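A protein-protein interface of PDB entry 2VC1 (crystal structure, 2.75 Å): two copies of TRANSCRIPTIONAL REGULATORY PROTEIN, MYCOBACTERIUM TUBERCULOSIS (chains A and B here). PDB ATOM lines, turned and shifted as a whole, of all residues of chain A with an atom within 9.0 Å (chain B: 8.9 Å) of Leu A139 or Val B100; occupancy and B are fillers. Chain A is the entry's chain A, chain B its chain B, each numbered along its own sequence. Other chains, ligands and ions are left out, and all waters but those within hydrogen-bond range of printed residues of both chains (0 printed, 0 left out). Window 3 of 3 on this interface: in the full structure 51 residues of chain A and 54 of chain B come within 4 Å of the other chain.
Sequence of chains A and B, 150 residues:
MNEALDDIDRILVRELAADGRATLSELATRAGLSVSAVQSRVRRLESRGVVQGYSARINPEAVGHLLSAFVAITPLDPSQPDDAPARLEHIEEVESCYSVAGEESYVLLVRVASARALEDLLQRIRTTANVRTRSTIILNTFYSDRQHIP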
ATOM      1  N   GLU A  61      -9.489   9.035   0.355  1.00  0.00           N
ATOM      2  CA  GLU A  61      -8.835  10.165  -0.283  1.00  0.00           C
ATOM      3  C   GLU A  61      -8.772  11.310   0.675  1.00  0.00           C
ATOM      4  O   GLU A  61      -7.685  11.841   0.913  1.00  0.00           O
ATOM      5  CB  GLU A  61      -9.670  10.648  -1.429  1.00  0.00           C
ATOM      6  CG  GLU A  61      -8.893  10.955  -2.675  1.00  0.00           C
ATOM      7  CD  GLU A  61      -9.471  10.169  -3.874  1.00  0.00           C
ATOM      8  OE1 GLU A  61     -10.222  10.795  -4.694  1.00  0.00           O
ATOM      9  OE2 GLU A  61      -9.199   8.927  -3.963  1.00  0.00           O
ATOM     10  N   LEU A  66      -4.246   8.262  -0.588  1.00  0.00           N
ATOM     11  CA  LEU A  66      -4.393   8.476  -2.018  1.00  0.00           C
ATOM     12  C   LEU A  66      -4.032   7.269  -2.918  1.00  0.00           C
ATOM     13  O   LEU A  66      -4.378   7.272  -4.107  1.00  0.00           O
ATOM     14  CB  LEU A  66      -3.599   9.698  -2.408  1.00  0.00           C
ATOM     15  CG  LEU A  66      -3.660  10.833  -1.357  1.00  0.00           C
ATOM     16  CD1 LEU A  66      -2.439  11.802  -1.481  1.00  0.00           C
ATOM     17  CD2 LEU A  66      -4.976  11.592  -1.428  1.00  0.00           C
ATOM     18  N   LEU A  67      -3.369   6.235  -2.372  1.00  0.00           N
ATOM     19  CA  LEU A  67      -3.086   4.981  -3.087  1.00  0.00           C
ATOM     20  C   LEU A  67      -3.682   3.772  -2.359  1.00  0.00           C
ATOM     21  O   LEU A  67      -3.448   3.587  -1.198  1.00  0.00           O
ATOM     22  CB  LEU A  67      -1.583   4.731  -3.119  1.00  0.00           C
ATOM     23  CG  LEU A  67      -0.881   4.534  -4.454  1.00  0.00           C
ATOM     24  CD1 LEU A  67       0.136   3.483  -4.311  1.00  0.00           C
ATOM     25  CD2 LEU A  67      -1.830   4.116  -5.477  1.00  0.00           C
ATOM     26  N   SER A  68      -4.371   2.914  -3.078  1.00  0.00           N
ATOM     27  CA  SER A  68      -4.993   1.728  -2.564  1.00  0.00           C
ATOM     28  C   SER A  68      -4.562   0.522  -3.411  1.00  0.00           C
ATOM     29  O   SER A  68      -4.420   0.654  -4.644  1.00  0.00           O
ATOM     30  CB  SER A  68      -6.495   1.889  -2.764  1.00  0.00           C
ATOM     31  OG  SER A  68      -6.990   2.480  -1.614  1.00  0.00           O
ATOM     32  N   ALA A  69      -4.417  -0.643  -2.787  1.00  0.00           N
ATOM     33  CA  ALA A  69      -4.019  -1.746  -3.592  1.00  0.00           C
ATOM     34  C   ALA A  69      -4.499  -3.091  -3.084  1.00  0.00           C
ATOM     35  O   ALA A  69      -4.827  -3.245  -1.877  1.00  0.00           O
ATOM     36  CB  ALA A  69      -2.481  -1.735  -3.839  1.00  0.00           C
ATOM     37  N   PHE A  70      -4.545  -4.043  -4.010  1.00  0.00           N
ATOM     38  CA  PHE A  70      -4.824  -5.401  -3.646  1.00  0.00           C
ATOM     39  C   PHE A  70      -3.494  -6.051  -3.556  1.00  0.00           C
ATOM     40  O   PHE A  70      -2.668  -5.924  -4.474  1.00  0.00           O
ATOM     41  CB  PHE A  70      -5.637  -6.114  -4.694  1.00  0.00           C
ATOM     42  CG  PHE A  70      -7.077  -5.772  -4.648  1.00  0.00           C
ATOM     43  CD1 PHE A  70      -7.677  -5.032  -5.700  1.00  0.00           C
ATOM     44  CD2 PHE A  70      -7.853  -6.108  -3.541  1.00  0.00           C
ATOM     45  CE1 PHE A  70      -9.026  -4.703  -5.628  1.00  0.00           C
ATOM     46  CE2 PHE A  70      -9.201  -5.765  -3.473  1.00  0.00           C
ATOM     47  CZ  PHE A  70      -9.788  -5.062  -4.525  1.00  0.00           C
ATOM     48  N   LEU A 109      -6.562  -5.945   1.130  1.00  0.00           N
ATOM     49  CA  LEU A 109      -6.752  -4.626   0.582  1.00  0.00           C
ATOM     50  C   LEU A 109      -6.054  -3.700   1.553  1.00  0.00           C
ATOM     51  O   LEU A 109      -6.269  -3.761   2.745  1.00  0.00           O
ATOM     52  CB  LEU A 109      -8.243  -4.262   0.420  1.00  0.00           C
ATOM     53  CG  LEU A 109      -8.455  -2.808   0.057  1.00  0.00           C
ATOM     54  CD1 LEU A 109      -8.324  -2.683  -1.358  1.00  0.00           C
ATOM     55  CD2 LEU A 109      -9.838  -2.472   0.387  1.00  0.00           C
ATOM     56  N   ARG A 134       1.926 -10.150  -4.461  1.00  0.00           N
ATOM     57  CA  ARG A 134       1.704  -9.661  -5.840  1.00  0.00           C
ATOM     58  C   ARG A 134       0.753  -8.451  -5.657  1.00  0.00           C
ATOM     59  O   ARG A 134      -0.197  -8.539  -4.900  1.00  0.00           O
ATOM     60  CB  ARG A 134       1.184 -10.746  -6.716  1.00  0.00           C
ATOM     61  CG  ARG A 134       0.759 -10.270  -8.091  1.00  0.00           C
ATOM     62  CD  ARG A 134       0.346 -11.391  -9.085  1.00  0.00           C
ATOM     63  NE  ARG A 134      -0.683 -12.267  -8.540  1.00  0.00           N
ATOM     64  CZ  ARG A 134      -2.015 -11.994  -8.510  1.00  0.00           C
ATOM     65  NH1 ARG A 134      -2.499 -10.877  -8.985  1.00  0.00           N
ATOM     66  NH2 ARG A 134      -2.881 -12.859  -7.978  1.00  0.00           N
ATOM     67  N   SER A 135       1.090  -7.288  -6.229  1.00  0.00           N
ATOM     68  CA  SER A 135       0.356  -6.032  -5.939  1.00  0.00           C
ATOM     69  C   SER A 135      -0.452  -5.645  -7.108  1.00  0.00           C
ATOM     70  O   SER A 135       0.080  -5.720  -8.180  1.00  0.00           O
ATOM     71  CB  SER A 135       1.331  -4.913  -5.701  1.00  0.00           C
ATOM     72  OG  SER A 135       1.813  -5.149  -4.427  1.00  0.00           O
ATOM     73  N   THR A 136      -1.693  -5.202  -6.895  1.00  0.00           N
ATOM     74  CA  THR A 136      -2.530  -4.634  -7.946  1.00  0.00           C
ATOM     75  C   THR A 136      -3.128  -3.355  -7.441  1.00  0.00           C
ATOM     76  O   THR A 136      -4.014  -3.360  -6.543  1.00  0.00           O
ATOM     77  CB  THR A 136      -3.621  -5.601  -8.275  1.00  0.00           C
ATOM     78  OG1 THR A 136      -2.995  -6.836  -8.624  1.00  0.00           O
ATOM     79  CG2 THR A 136      -4.402  -5.168  -9.433  1.00  0.00           C
ATOM     80  N   ILE A 137      -2.574  -2.257  -7.957  1.00  0.00           N
ATOM     81  CA  ILE A 137      -2.921  -0.866  -7.556  1.00  0.00           C
ATOM     82  C   ILE A 137      -4.287  -0.592  -8.129  1.00  0.00           C
ATOM     83  O   ILE A 137      -4.565  -0.929  -9.268  1.00  0.00           O
ATOM     84  CB  ILE A 137      -1.981   0.160  -8.210  1.00  0.00           C
ATOM     85  CG1 ILE A 137      -0.507  -0.109  -7.868  1.00  0.00           C
ATOM     86  CG2 ILE A 137      -2.368   1.526  -7.944  1.00  0.00           C
ATOM     87  CD1 ILE A 137      -0.174   0.029  -6.509  1.00  0.00           C
ATOM     88  N   ILE A 138      -5.144  -0.014  -7.307  1.00  0.00           N
ATOM     89  CA  ILE A 138      -6.434   0.390  -7.760  1.00  0.00           C
ATOM     90  C   ILE A 138      -6.344   1.766  -8.387  1.00  0.00           C
ATOM     91  O   ILE A 138      -5.677   2.600  -7.821  1.00  0.00           O
ATOM     92  CB  ILE A 138      -7.300   0.413  -6.579  1.00  0.00           C
ATOM     93  CG1 ILE A 138      -7.420  -1.044  -6.110  1.00  0.00           C
ATOM     94  CG2 ILE A 138      -8.610   1.237  -6.903  1.00  0.00           C
ATOM     95  CD1 ILE A 138      -8.186  -1.169  -4.735  1.00  0.00           C
ATOM     96  N   LEU A 139      -6.957   2.013  -9.541  1.00  0.00           N
ATOM     97  CA  LEU A 139      -6.803   3.327 -10.251  1.00  0.00           C
ATOM     98  C   LEU A 139      -7.942   4.226  -9.877  1.00  0.00           C
ATOM     99  O   LEU A 139      -7.762   5.454  -9.758  1.00  0.00           O
ATOM    100  CB  LEU A 139      -6.822   3.175 -11.763  1.00  0.00           C
ATOM    101  CG  LEU A 139      -5.623   2.342 -12.279  1.00  0.00           C
ATOM    102  CD1 LEU A 139      -5.586   2.182 -13.747  1.00  0.00           C
ATOM    103  CD2 LEU A 139      -4.271   2.858 -11.745  1.00  0.00           C
ATOM    104  N   ASN A 140      -9.121   3.599  -9.699  1.00  0.00           N
ATOM    105  CA  ASN A 140     -10.365   4.209  -9.355  1.00  0.00           C
ATOM    106  C   ASN A 140     -11.423   3.252  -8.748  1.00  0.00           C
ATOM    107  O   ASN A 140     -11.594   2.131  -9.259  1.00  0.00           O
ATOM    108  CB  ASN A 140     -10.915   4.739 -10.636  1.00  0.00           C
ATOM    109  CG  ASN A 140     -12.163   5.600 -10.400  1.00  0.00           C
ATOM    110  OD1 ASN A 140     -12.255   6.342  -9.399  1.00  0.00           O
ATOM    111  ND2 ASN A 140     -13.161   5.453 -11.299  1.00  0.00           N
ATOM    112  N   THR A 141     -12.134   3.644  -7.682  1.00  0.00           N
ATOM    113  CA  THR A 141     -13.278   2.884  -7.165  1.00  0.00           C
ATOM    114  C   THR A 141     -14.573   3.418  -7.788  1.00  0.00           C
ATOM    115  O   THR A 141     -14.850   4.523  -7.555  1.00  0.00           O
ATOM    116  CB  THR A 141     -13.425   3.086  -5.696  1.00  0.00           C
ATOM    117  OG1 THR A 141     -12.282   2.536  -5.074  1.00  0.00           O
ATOM    118  CG2 THR A 141     -14.564   2.305  -5.132  1.00  0.00           C
ATOM    119  N   PHE A 142     -15.380   2.648  -8.532  1.00  0.00           N
ATOM    120  CA  PHE A 142     -16.621   3.153  -9.052  1.00  0.00           C
ATOM    121  C   PHE A 142     -17.776   3.123  -8.050  1.00  0.00           C
ATOM    122  O   PHE A 142     -18.662   3.985  -8.124  1.00  0.00           O
ATOM    123  CB  PHE A 142     -17.007   2.453 -10.340  1.00  0.00           C
ATOM    124  CG  PHE A 142     -16.035   2.682 -11.419  1.00  0.00           C
ATOM    125  CD1 PHE A 142     -16.204   3.746 -12.308  1.00  0.00           C
ATOM    126  CD2 PHE A 142     -14.844   1.909 -11.484  1.00  0.00           C
ATOM    127  CE1 PHE A 142     -15.195   4.034 -13.262  1.00  0.00           C
ATOM    128  CE2 PHE A 142     -13.874   2.145 -12.463  1.00  0.00           C
ATOM    129  CZ  PHE A 142     -14.045   3.223 -13.353  1.00  0.00           C
ATOM    130  N   VAL B  71     -13.939 -11.028  -9.084  1.00  0.00           N
ATOM    131  CA  VAL B  71     -14.050 -11.459 -10.453  1.00  0.00           C
ATOM    132  C   VAL B  71     -13.342 -10.406 -11.246  1.00  0.00           C
ATOM    133  O   VAL B  71     -13.670  -9.237 -11.153  1.00  0.00           O
ATOM    134  CB  VAL B  71     -15.478 -11.465 -10.916  1.00  0.00           C
ATOM    135  CG1 VAL B  71     -15.543 -11.702 -12.374  1.00  0.00           C
ATOM    136  CG2 VAL B  71     -16.241 -12.436 -10.171  1.00  0.00           C
ATOM    137  N   ALA B  72     -12.356 -10.793 -12.009  1.00  0.00           N
ATOM    138  CA  ALA B  72     -11.514  -9.845 -12.652  1.00  0.00           C
ATOM    139  C   ALA B  72     -12.051  -9.824 -14.069  1.00  0.00           C
ATOM    140  O   ALA B  72     -12.182 -10.901 -14.700  1.00  0.00           O
ATOM    141  CB  ALA B  72     -10.060 -10.354 -12.632  1.00  0.00           C
ATOM    142  N   ILE B  73     -12.322  -8.662 -14.615  1.00  0.00           N
ATOM    143  CA  ILE B  73     -12.837  -8.632 -15.990  1.00  0.00           C
ATOM    144  C   ILE B  73     -12.021  -7.721 -16.879  1.00  0.00           C
ATOM    145  O   ILE B  73     -11.352  -6.772 -16.432  1.00  0.00           O
ATOM    146  CB  ILE B  73     -14.307  -8.125 -16.047  1.00  0.00           C
ATOM    147  CG1 ILE B  73     -14.403  -6.721 -15.473  1.00  0.00           C
ATOM    148  CG2 ILE B  73     -15.260  -8.981 -15.180  1.00  0.00           C
ATOM    149  CD1 ILE B  73     -15.694  -6.160 -15.526  1.00  0.00           C
ATOM    150  N   THR B  74     -12.075  -8.002 -18.159  1.00  0.00           N
ATOM    151  CA  THR B  74     -11.391  -7.220 -19.183  1.00  0.00           C
ATOM    152  C   THR B  74     -12.314  -7.205 -20.419  1.00  0.00           C
ATOM    153  O   THR B  74     -12.689  -8.270 -20.891  1.00  0.00           O
ATOM    154  CB  THR B  74     -10.211  -8.000 -19.651  1.00  0.00           C
ATOM    155  OG1 THR B  74      -9.340  -8.202 -18.554  1.00  0.00           O
ATOM    156  CG2 THR B  74      -9.472  -7.304 -20.800  1.00  0.00           C
ATOM    157  N   CYS B  97     -16.755  -2.336  -7.488  1.00  0.00           N
ATOM    158  CA  CYS B  97     -16.131  -2.401  -8.783  1.00  0.00           C
ATOM    159  C   CYS B  97     -14.959  -1.397  -8.886  1.00  0.00           C
ATOM    160  O   CYS B  97     -15.116  -0.199  -8.613  1.00  0.00           O
ATOM    161  CB  CYS B  97     -17.170  -2.149  -9.794  1.00  0.00           C
ATOM    162  SG  CYS B  97     -16.503  -1.856 -11.370  1.00  0.00           S
ATOM    163  N   TYR B  98     -13.771  -1.892  -9.197  1.00  0.00           N
ATOM    164  CA  TYR B  98     -12.554  -1.056  -9.198  1.00  0.00           C
ATOM    165  C   TYR B  98     -11.893  -1.118 -10.558  1.00  0.00           C
ATOM    166  O   TYR B  98     -11.877  -2.215 -11.180  1.00  0.00           O
ATOM    167  CB  TYR B  98     -11.540  -1.604  -8.218  1.00  0.00           C
ATOM    168  CG  TYR B  98     -12.041  -1.829  -6.822  1.00  0.00           C
ATOM    169  CD1 TYR B  98     -12.554  -3.099  -6.376  1.00  0.00           C
ATOM    170  CD2 TYR B  98     -11.983  -0.763  -5.913  1.00  0.00           C
ATOM    171  CE1 TYR B  98     -13.047  -3.260  -5.029  1.00  0.00           C
ATOM    172  CE2 TYR B  98     -12.468  -0.887  -4.611  1.00  0.00           C
ATOM    173  CZ  TYR B  98     -12.984  -2.103  -4.176  1.00  0.00           C
ATOM    174  OH  TYR B  98     -13.383  -2.043  -2.875  1.00  0.00           O
ATOM    175  N   SER B  99     -11.370   0.000 -11.060  1.00  0.00           N
ATOM    176  CA  SER B  99     -10.444  -0.174 -12.161  1.00  0.00           C
ATOM    177  C   SER B  99      -9.114  -0.432 -11.534  1.00  0.00           C
ATOM    178  O   SER B  99      -8.794   0.042 -10.419  1.00  0.00           O
ATOM    179  CB  SER B  99     -10.335   1.003 -13.080  1.00  0.00           C
ATOM    180  OG  SER B  99      -9.903   2.081 -12.277  1.00  0.00           O
ATOM    181  N   VAL B 100      -8.302  -1.179 -12.236  1.00  0.00           N
ATOM    182  CA  VAL B 100      -7.109  -1.751 -11.576  1.00  0.00           C
ATOM    183  C   VAL B 100      -5.931  -1.623 -12.551  1.00  0.00           C
ATOM    184  O   VAL B 100      -6.166  -1.412 -13.761  1.00  0.00           O
ATOM    185  CB  VAL B 100      -7.525  -3.161 -11.115  1.00  0.00           C
ATOM    186  CG1 VAL B 100      -6.941  -4.207 -11.902  1.00  0.00           C
ATOM    187  CG2 VAL B 100      -7.495  -3.277  -9.660  1.00  0.00           C
ATOM    188  N   ALA B 101      -4.695  -1.656 -12.043  1.00  0.00           N
ATOM    189  CA  ALA B 101      -3.450  -1.679 -12.917  1.00  0.00           C
ATOM    190  C   ALA B 101      -2.842  -3.005 -12.716  1.00  0.00           C
ATOM    191  O   ALA B 101      -2.155  -3.230 -11.728  1.00  0.00           O
ATOM    192  CB  ALA B 101      -2.465  -0.652 -12.512  1.00  0.00           C
ATOM    193  N   GLY B 102      -3.112  -3.900 -13.634  1.00  0.00           N
ATOM    194  CA  GLY B 102      -2.839  -5.301 -13.485  1.00  0.00           C
ATOM    195  C   GLY B 102      -2.916  -6.041 -14.797  1.00  0.00           C
ATOM    196  O   GLY B 102      -2.498  -5.471 -15.837  1.00  0.00           O
ATOM    197  N   GLU B 103      -3.374  -7.325 -14.730  1.00  0.00           N
ATOM    198  CA  GLU B 103      -3.667  -8.118 -15.970  1.00  0.00           C
ATOM    199  C   GLU B 103      -5.052  -7.823 -16.562  1.00  0.00           C
ATOM    200  O   GLU B 103      -5.248  -7.826 -17.793  1.00  0.00           O
ATOM    201  CB  GLU B 103      -3.638  -9.578 -15.731  1.00  0.00           C
ATOM    202  CG  GLU B 103      -2.459 -10.177 -14.997  1.00  0.00           C
ATOM    203  CD  GLU B 103      -2.211 -11.595 -15.576  1.00  0.00           C
ATOM    204  OE1 GLU B 103      -2.546 -11.828 -16.800  1.00  0.00           O
ATOM    205  OE2 GLU B 103      -1.685 -12.448 -14.822  1.00  0.00           O
ATOM    206  N   GLU B 104      -6.011  -7.587 -15.674  1.00  0.00           N
ATOM    207  CA  GLU B 104      -7.389  -7.277 -15.981  1.00  0.00           C
ATOM    208  C   GLU B 104      -7.655  -5.739 -15.929  1.00  0.00           C
ATOM    209  O   GLU B 104      -6.813  -4.974 -15.454  1.00  0.00           O
ATOM    210  CB  GLU B 104      -8.235  -8.069 -14.981  1.00  0.00           C
ATOM    211  CG  GLU B 104      -9.103  -9.253 -15.582  1.00  0.00           C
ATOM    212  CD  GLU B 104      -8.365 -10.404 -16.443  1.00  0.00           C
ATOM    213  OE1 GLU B 104      -7.408 -11.119 -15.957  1.00  0.00           O
ATOM    214  OE2 GLU B 104      -8.843 -10.621 -17.609  1.00  0.00           O
ATOM    215  N   SER B 105      -8.809  -5.265 -16.423  1.00  0.00           N
ATOM    216  CA  SER B 105      -9.108  -3.889 -16.343  1.00  0.00           C
ATOM    217  C   SER B 105      -9.846  -3.603 -15.059  1.00  0.00           C
ATOM    218  O   SER B 105      -9.700  -2.533 -14.530  1.00  0.00           O
ATOM    219  CB  SER B 105     -10.013  -3.497 -17.467  1.00  0.00           C
ATOM    220  OG  SER B 105      -9.426  -3.591 -18.732  1.00  0.00           O
ATOM    221  N   TYR B 106     -10.681  -4.538 -14.583  1.00  0.00           N
ATOM    222  CA  TYR B 106     -11.440  -4.266 -13.390  1.00  0.00           C
ATOM    223  C   TYR B 106     -11.443  -5.452 -12.466  1.00  0.00           C
ATOM    224  O   TYR B 106     -11.392  -6.571 -13.014  1.00  0.00           O
ATOM    225  CB  TYR B 106     -12.858  -3.951 -13.795  1.00  0.00           C
ATOM    226  CG  TYR B 106     -12.990  -2.798 -14.754  1.00  0.00           C
ATOM    227  CD1 TYR B 106     -13.058  -1.471 -14.311  1.00  0.00           C
ATOM    228  CD2 TYR B 106     -13.185  -3.024 -16.118  1.00  0.00           C
ATOM    229  CE1 TYR B 106     -13.294  -0.435 -15.218  1.00  0.00           C
ATOM    230  CE2 TYR B 106     -13.355  -2.037 -16.998  1.00  0.00           C
ATOM    231  CZ  TYR B 106     -13.423  -0.741 -16.561  1.00  0.00           C
ATOM    232  OH  TYR B 106     -13.600   0.244 -17.523  1.00  0.00           O
ATOM    233  N   VAL B 107     -11.620  -5.208 -11.146  1.00  0.00           N
ATOM    234  CA  VAL B 107     -11.953  -6.247 -10.188  1.00  0.00           C
ATOM    235  C   VAL B 107     -13.367  -6.011  -9.649  1.00  0.00           C
ATOM    236  O   VAL B 107     -13.685  -4.867  -9.342  1.00  0.00           O
ATOM    237  CB  VAL B 107     -10.840  -6.316  -9.132  1.00  0.00           C
ATOM    238  CG1 VAL B 107     -11.150  -7.357  -8.019  1.00  0.00           C
ATOM    239  CG2 VAL B 107      -9.550  -6.664  -9.872  1.00  0.00           C
ATOM    240  N   LEU B 108     -14.215  -7.063  -9.568  1.00  0.00           N
ATOM    241  CA  LEU B 108     -15.499  -6.958  -8.871  1.00  0.00           C
ATOM    242  C   LEU B 108     -15.444  -7.780  -7.605  1.00  0.00           C
ATOM    243  O   LEU B 108     -14.752  -8.810  -7.556  1.00  0.00           O
ATOM    244  CB  LEU B 108     -16.554  -7.499  -9.757  1.00  0.00           C
ATOM    245  CG  LEU B 108     -16.556  -7.029 -11.184  1.00  0.00           C
ATOM    246  CD1 LEU B 108     -17.791  -7.636 -11.900  1.00  0.00           C
ATOM    247  CD2 LEU B 108     -16.547  -5.464 -11.372  1.00  0.00           C
ATOM    248  N   ARG B 134     -12.396 -13.666 -14.896  1.00  0.00           N
ATOM    249  CA  ARG B 134     -11.459 -14.644 -14.353  1.00  0.00           C
ATOM    250  C   ARG B 134     -11.730 -14.546 -12.880  1.00  0.00           C
ATOM    251  O   ARG B 134     -11.594 -13.467 -12.276  1.00  0.00           O
ATOM    252  CB  ARG B 134      -9.967 -14.380 -14.747  1.00  0.00           C
ATOM    253  CG  ARG B 134      -8.921 -14.966 -13.792  1.00  0.00           C
ATOM    254  CD  ARG B 134      -7.400 -14.777 -14.269  1.00  0.00           C
ATOM    255  NE  ARG B 134      -6.944 -13.369 -14.443  1.00  0.00           N
ATOM    256  CZ  ARG B 134      -6.653 -12.535 -13.404  1.00  0.00           C
ATOM    257  NH1 ARG B 134      -6.770 -12.995 -12.105  1.00  0.00           N
ATOM    258  NH2 ARG B 134      -6.269 -11.221 -13.627  1.00  0.00           N
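The backbone carbonyl oxygen (O) of Asn A140 is in hydrogen-bond range of the backbone NH (N) of Ser B99 (2.8 Å). N of Ala B101 sits at hydrogen-bond distance from O of Ile A137. The backbone NH (N) of Phe A142 is in hydrogen-bond range of the backbone carbonyl oxygen (O) of Cys B97 (2.9 Å). N of Leu A139 sits at hydrogen-bond distance from O of Ser B99 (2.8 Å).
N of Val B100 lies within hydrogen-bond range of O of Ser B105 (3.0 Å). The backbone NH (N) of Ile B73 sits at hydrogen-bond distance from the backbone carbonyl oxygen (O) of Tyr B106, 2.8 Å away. O of Thr A136 lies within hydrogen-bond range of N of Phe A70, at 2.7 Å. O of Val B107 sits at hydrogen-bond distance from N of Tyr B98. The backbone carbonyl oxygen (O) of Ser A68 sits at hydrogen-bond distance from the backbone NH (N) of Ile A138 (2.8 Å).
CE1 of Tyr B98 touches CZ of Phe A70, at 3.8 Å. Thr A136 touches Ala B101. Ile A137 touches Val B100 (O to CA, 3.5 Å). CD2 of Tyr B98 touches CD1 of Ile A138, 3.996 Å away. CA of Ile A138 touches O of Ser B99, 3.6 Å away. Asn A140 touches Tyr B98. Thr A141 touches Cys B97 (C to O, 3.7 Å). Tyr B98 touches Thr A141. Phe A142 touches Ser B99. Tyr B106 touches Phe A142 (CE1 to CE2, 3.8 Å).
Glu A61 touches none of the printed residues of chain B. Printed residues of chain B within 4 Å of Phe A70: Tyr B98. Arg A134 touches none of the printed residues of chain B. Printed residues of chain B within 4 Å of Leu A139: Ser B99 (2.8 Å) and Val B100 (3.6 Å). Of the printed residues of chain A, Cys B97 touches Thr A141 (3.7 Å) and Phe A142 (2.9 Å). Of chain A, only Thr A136, Ile A137 and Leu A139 come within 4 Å of Val B100. Of chain A, only Thr A136 (3.8 Å) and Ile A137 (2.9 Å) come within 4 Å of Ala B101. The nearest residue of chain B that does not touch Leu A139 is Ala B101 (4.02 Å). The nearest residue of chain A that does not touch Val B100 is Ile A138 (4.2 Å).
Of the 17 printed residues of chain B, 6 touch a printed residue of chain A. Hydrophobic or aromatic side chains of chain B within 4 Å of the printed part of chain A: Tyr B98, Val B100, Ala B101 and Tyr B106. Of the 16 printed residues of chain A, 8 touch a printed residue of chain B. Hydrophobic or aromatic side chains of chain A that line the printed part of chain B: Phe A70, Ile A138, Leu A139 and Phe A142. Among the printed residues, 16 pairs touch across the chains. Among the printed residues, no Asp or Glu carboxylate lies within 4 Å of a Lys or Arg side-chain nitrogen of the other chain.
1 position is printed for both chains.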
